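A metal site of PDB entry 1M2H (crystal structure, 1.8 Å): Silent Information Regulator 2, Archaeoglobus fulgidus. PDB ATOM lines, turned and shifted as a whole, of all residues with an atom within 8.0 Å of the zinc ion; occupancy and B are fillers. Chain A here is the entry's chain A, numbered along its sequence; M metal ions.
SG of Cys 124 is bound to the zinc ion (2.3 Å). The side-chain sulfur (SG) of Cys 148 is bound to the zinc ion. The side-chain sulfur (SG) of Cys 145 is bound to the zinc ion, at 2.3 Å. SG of Cys 127 is bound to the zinc ion, at 2.3 Å.
OG of Ser 150 touches the zinc ion, at 3.4 Å. Of the 17 residues printed, 5 come within 4 Å of the zinc ion. The nearest printed residue that does not touch the zinc ion is Lys 147 (4.3 Å).
OG of Ser 150 sits close to SG of Cys 124. The backbone NH of Cys 124 lies within hydrogen-bond range of the backbone carbonyl oxygen of Asn 129. SG of Cys 124 lies close to N of Ser 126. SG of Cys 148 sits close to OG of Ser 150, at 2.8 Å. The backbone carbonyl oxygen (O) of Ser 150 lies within hydrogen-bond range of the backbone NH (N) of Cys 145, 2.8 Å away. The side-chain sulfur (SG) of Cys 145 sits close to the backbone NH (N) of Lys 147. SG of Cys 127 sits close to N of Asn 129 (3.5 Å). The side-chain hydroxyl (OG) of Ser 150 lies close to the side-chain hydroxyl (OG) of Ser 126.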
ATOM      1  N   ARG A 123      -5.480 -29.004 -25.391  1.00  0.00           N
ATOM      2  CA  ARG A 123      -6.436 -28.149 -24.702  1.00  0.00           C
ATOM      3  C   ARG A 123      -6.814 -28.686 -23.336  1.00  0.00           C
ATOM      4  O   ARG A 123      -6.634 -29.872 -23.047  1.00  0.00           O
ATOM      5  CB  ARG A 123      -7.699 -27.965 -25.546  1.00  0.00           C
ATOM      6  CG  ARG A 123      -8.521 -29.228 -25.751  1.00  0.00           C
ATOM      7  CD  ARG A 123      -9.661 -28.972 -26.711  1.00  0.00           C
ATOM      8  NE  ARG A 123     -10.484 -30.163 -26.922  1.00  0.00           N
ATOM      9  CZ  ARG A 123     -11.296 -30.678 -26.006  1.00  0.00           C
ATOM     10  NH1 ARG A 123     -11.392 -30.127 -24.805  1.00  0.00           N
ATOM     11  NH2 ARG A 123     -12.024 -31.756 -26.290  1.00  0.00           N
ATOM     12  N   CYS A 124      -7.341 -27.803 -22.512  1.00  0.00           N
ATOM     13  CA  CYS A 124      -7.734 -28.167 -21.160  1.00  0.00           C
ATOM     14  C   CYS A 124      -9.049 -28.930 -21.162  1.00  0.00           C
ATOM     15  O   CYS A 124      -9.890 -28.737 -22.045  1.00  0.00           O
ATOM     16  CB  CYS A 124      -7.876 -26.910 -20.309  1.00  0.00           C
ATOM     17  SG  CYS A 124      -8.166 -27.254 -18.563  1.00  0.00           S
ATOM     18  N   THR A 125      -9.217 -29.806 -20.181  1.00  0.00           N
ATOM     19  CA  THR A 125     -10.435 -30.586 -20.063  1.00  0.00           C
ATOM     20  C   THR A 125     -11.457 -29.850 -19.197  1.00  0.00           C
ATOM     21  O   THR A 125     -12.600 -30.298 -19.061  1.00  0.00           O
ATOM     22  CB  THR A 125     -10.141 -31.950 -19.418  1.00  0.00           C
ATOM     23  OG1 THR A 125      -9.499 -31.761 -18.154  1.00  0.00           O
ATOM     24  CG2 THR A 125      -9.233 -32.775 -20.329  1.00  0.00           C
ATOM     25  N   SER A 126     -11.050 -28.722 -18.618  1.00  0.00           N
ATOM     26  CA  SER A 126     -11.930 -27.938 -17.750  1.00  0.00           C
ATOM     27  C   SER A 126     -12.225 -26.538 -18.276  1.00  0.00           C
ATOM     28  O   SER A 126     -13.379 -26.162 -18.463  1.00  0.00           O
ATOM     29  CB  SER A 126     -11.329 -27.826 -16.355  1.00  0.00           C
ATOM     30  OG  SER A 126     -11.150 -29.111 -15.785  1.00  0.00           O
ATOM     31  N   CYS A 127     -11.176 -25.738 -18.492  1.00  0.00           N
ATOM     32  CA  CYS A 127     -11.373 -24.384 -18.989  1.00  0.00           C
ATOM     33  C   CYS A 127     -11.149 -24.353 -20.495  1.00  0.00           C
ATOM     34  O   CYS A 127     -10.863 -25.376 -21.109  1.00  0.00           O
ATOM     35  CB  CYS A 127     -10.443 -23.404 -18.275  1.00  0.00           C
ATOM     36  SG  CYS A 127      -8.685 -23.479 -18.721  1.00  0.00           S
ATOM     37  N   ASN A 128     -11.272 -23.167 -21.088  1.00  0.00           N
ATOM     38  CA  ASN A 128     -11.131 -23.036 -22.541  1.00  0.00           C
ATOM     39  C   ASN A 128      -9.718 -22.832 -23.063  1.00  0.00           C
ATOM     40  O   ASN A 128      -9.519 -22.601 -24.258  1.00  0.00           O
ATOM     41  CB  ASN A 128     -12.035 -21.899 -23.036  1.00  0.00           C
ATOM     42  CG  ASN A 128     -12.168 -21.889 -24.546  1.00  0.00           C
ATOM     43  OD1 ASN A 128     -12.561 -22.887 -25.154  1.00  0.00           O
ATOM     44  ND2 ASN A 128     -11.854 -20.755 -25.158  1.00  0.00           N
ATOM     45  N   ASN A 129      -8.711 -22.927 -22.196  1.00  0.00           N
ATOM     46  CA  ASN A 129      -7.349 -22.741 -22.658  1.00  0.00           C
ATOM     47  C   ASN A 129      -6.924 -23.831 -23.634  1.00  0.00           C
ATOM     48  O   ASN A 129      -7.174 -25.023 -23.419  1.00  0.00           O
ATOM     49  CB  ASN A 129      -6.370 -22.697 -21.487  1.00  0.00           C
ATOM     50  CG  ASN A 129      -4.924 -22.534 -21.952  1.00  0.00           C
ATOM     51  OD1 ASN A 129      -4.356 -23.425 -22.580  1.00  0.00           O
ATOM     52  ND2 ASN A 129      -4.331 -21.394 -21.643  1.00  0.00           N
ATOM     53  N   SER A 130      -6.279 -23.421 -24.714  1.00  0.00           N
ATOM     54  CA  SER A 130      -5.775 -24.346 -25.720  1.00  0.00           C
ATOM     55  C   SER A 130      -4.567 -23.684 -26.357  1.00  0.00           C
ATOM     56  O   SER A 130      -4.401 -22.466 -26.284  1.00  0.00           O
ATOM     57  CB  SER A 130      -6.843 -24.628 -26.784  1.00  0.00           C
ATOM     58  OG  SER A 130      -6.984 -23.539 -27.680  1.00  0.00           O
ATOM     59  N   LYS A 144      -0.431 -30.659 -17.446  1.00  0.00           N
ATOM     60  CA  LYS A 144      -1.411 -29.902 -16.674  1.00  0.00           C
ATOM     61  C   LYS A 144      -1.574 -28.463 -17.141  1.00  0.00           C
ATOM     62  O   LYS A 144      -0.608 -27.792 -17.523  1.00  0.00           O
ATOM     63  CB  LYS A 144      -1.035 -29.941 -15.194  1.00  0.00           C
ATOM     64  CG  LYS A 144      -1.150 -31.324 -14.569  1.00  0.00           C
ATOM     65  CD  LYS A 144      -0.809 -31.299 -13.086  1.00  0.00           C
ATOM     66  CE  LYS A 144      -0.938 -32.685 -12.461  1.00  0.00           C
ATOM     67  NZ  LYS A 144      -2.305 -33.242 -12.619  1.00  0.00           N
ATOM     68  N   CYS A 145      -2.814 -28.001 -17.105  1.00  0.00           N
ATOM     69  CA  CYS A 145      -3.165 -26.648 -17.518  1.00  0.00           C
ATOM     70  C   CYS A 145      -2.515 -25.571 -16.649  1.00  0.00           C
ATOM     71  O   CYS A 145      -2.583 -25.626 -15.422  1.00  0.00           O
ATOM     72  CB  CYS A 145      -4.679 -26.499 -17.489  1.00  0.00           C
ATOM     73  SG  CYS A 145      -5.284 -24.865 -18.007  1.00  0.00           S
ATOM     74  N   ASP A 146      -1.904 -24.588 -17.295  1.00  0.00           N
ATOM     75  CA  ASP A 146      -1.234 -23.506 -16.584  1.00  0.00           C
ATOM     76  C   ASP A 146      -2.229 -22.426 -16.173  1.00  0.00           C
ATOM     77  O   ASP A 146      -1.850 -21.407 -15.596  1.00  0.00           O
ATOM     78  CB  ASP A 146      -0.144 -22.896 -17.476  1.00  0.00           C
ATOM     79  CG  ASP A 146      -0.706 -22.188 -18.706  1.00  0.00           C
ATOM     80  OD1 ASP A 146      -1.303 -21.106 -18.546  1.00  0.00           O
ATOM     81  OD2 ASP A 146      -0.552 -22.717 -19.823  1.00  0.00           O
ATOM     82  N   LYS A 147      -3.508 -22.649 -16.463  1.00  0.00           N
ATOM     83  CA  LYS A 147      -4.547 -21.684 -16.111  1.00  0.00           C
ATOM     84  C   LYS A 147      -5.345 -22.084 -14.875  1.00  0.00           C
ATOM     85  O   LYS A 147      -5.612 -21.256 -14.007  1.00  0.00           O
ATOM     86  CB  LYS A 147      -5.499 -21.484 -17.292  1.00  0.00           C
ATOM     87  CG  LYS A 147      -4.848 -20.868 -18.520  1.00  0.00           C
ATOM     88  CD  LYS A 147      -4.266 -19.504 -18.205  1.00  0.00           C
ATOM     89  CE  LYS A 147      -3.597 -18.904 -19.436  1.00  0.00           C
ATOM     90  NZ  LYS A 147      -3.009 -17.569 -19.125  1.00  0.00           N
ATOM     91  N   CYS A 148      -5.723 -23.356 -14.795  1.00  0.00           N
ATOM     92  CA  CYS A 148      -6.495 -23.831 -13.656  1.00  0.00           C
ATOM     93  C   CYS A 148      -5.894 -25.072 -13.006  1.00  0.00           C
ATOM     94  O   CYS A 148      -6.358 -25.523 -11.959  1.00  0.00           O
ATOM     95  CB  CYS A 148      -7.930 -24.139 -14.094  1.00  0.00           C
ATOM     96  SG  CYS A 148      -8.039 -25.386 -15.403  1.00  0.00           S
ATOM     97  N   GLY A 149      -4.874 -25.642 -13.645  1.00  0.00           N
ATOM     98  CA  GLY A 149      -4.221 -26.808 -13.091  1.00  0.00           C
ATOM     99  C   GLY A 149      -4.867 -28.143 -13.412  1.00  0.00           C
ATOM    100  O   GLY A 149      -4.398 -29.187 -12.964  1.00  0.00           O
ATOM    101  N   SER A 150      -5.941 -28.124 -14.197  1.00  0.00           N
ATOM    102  CA  SER A 150      -6.616 -29.367 -14.555  1.00  0.00           C
ATOM    103  C   SER A 150      -5.862 -30.094 -15.663  1.00  0.00           C
ATOM    104  O   SER A 150      -4.965 -29.536 -16.303  1.00  0.00           O
ATOM    105  CB  SER A 150      -8.051 -29.088 -14.988  1.00  0.00           C
ATOM    106  OG  SER A 150      -8.089 -28.151 -16.046  1.00  0.00           O
ATOM    107  N   LEU A 151      -6.230 -31.353 -15.897  1.00  0.00           N
ATOM    108  CA  LEU A 151      -5.603 -32.180 -16.915  1.00  0.00           C
ATOM    109  C   LEU A 151      -5.803 -31.660 -18.337  1.00  0.00           C
ATOM    110  O   LEU A 151      -6.891 -31.226 -18.708  1.00  0.00           O
ATOM    111  CB  LEU A 151      -6.157 -33.603 -16.817  1.00  0.00           C
ATOM    112  CG  LEU A 151      -5.671 -34.679 -17.803  1.00  0.00           C
ATOM    113  CD1 LEU A 151      -4.193 -34.939 -17.599  1.00  0.00           C
ATOM    114  CD2 LEU A 151      -6.466 -35.962 -17.585  1.00  0.00           C
ATOM    115  N   LEU A 152      -4.732 -31.685 -19.131  1.00  0.00           N
ATOM    116  CA  LEU A 152      -4.819 -31.249 -20.522  1.00  0.00           C
ATOM    117  C   LEU A 152      -5.050 -32.516 -21.332  1.00  0.00           C
ATOM    118  O   LEU A 152      -4.846 -33.623 -20.821  1.00  0.00           O
ATOM    119  CB  LEU A 152      -3.514 -30.582 -20.967  1.00  0.00           C
ATOM    120  CG  LEU A 152      -3.119 -29.248 -20.334  1.00  0.00           C
ATOM    121  CD1 LEU A 152      -1.699 -28.882 -20.744  1.00  0.00           C
ATOM    122  CD2 LEU A 152      -4.095 -28.166 -20.759  1.00  0.00           C
HETATM  123 ZN    ZN M   1      -7.550 -25.221 -17.657  1.00  0.00          ZN
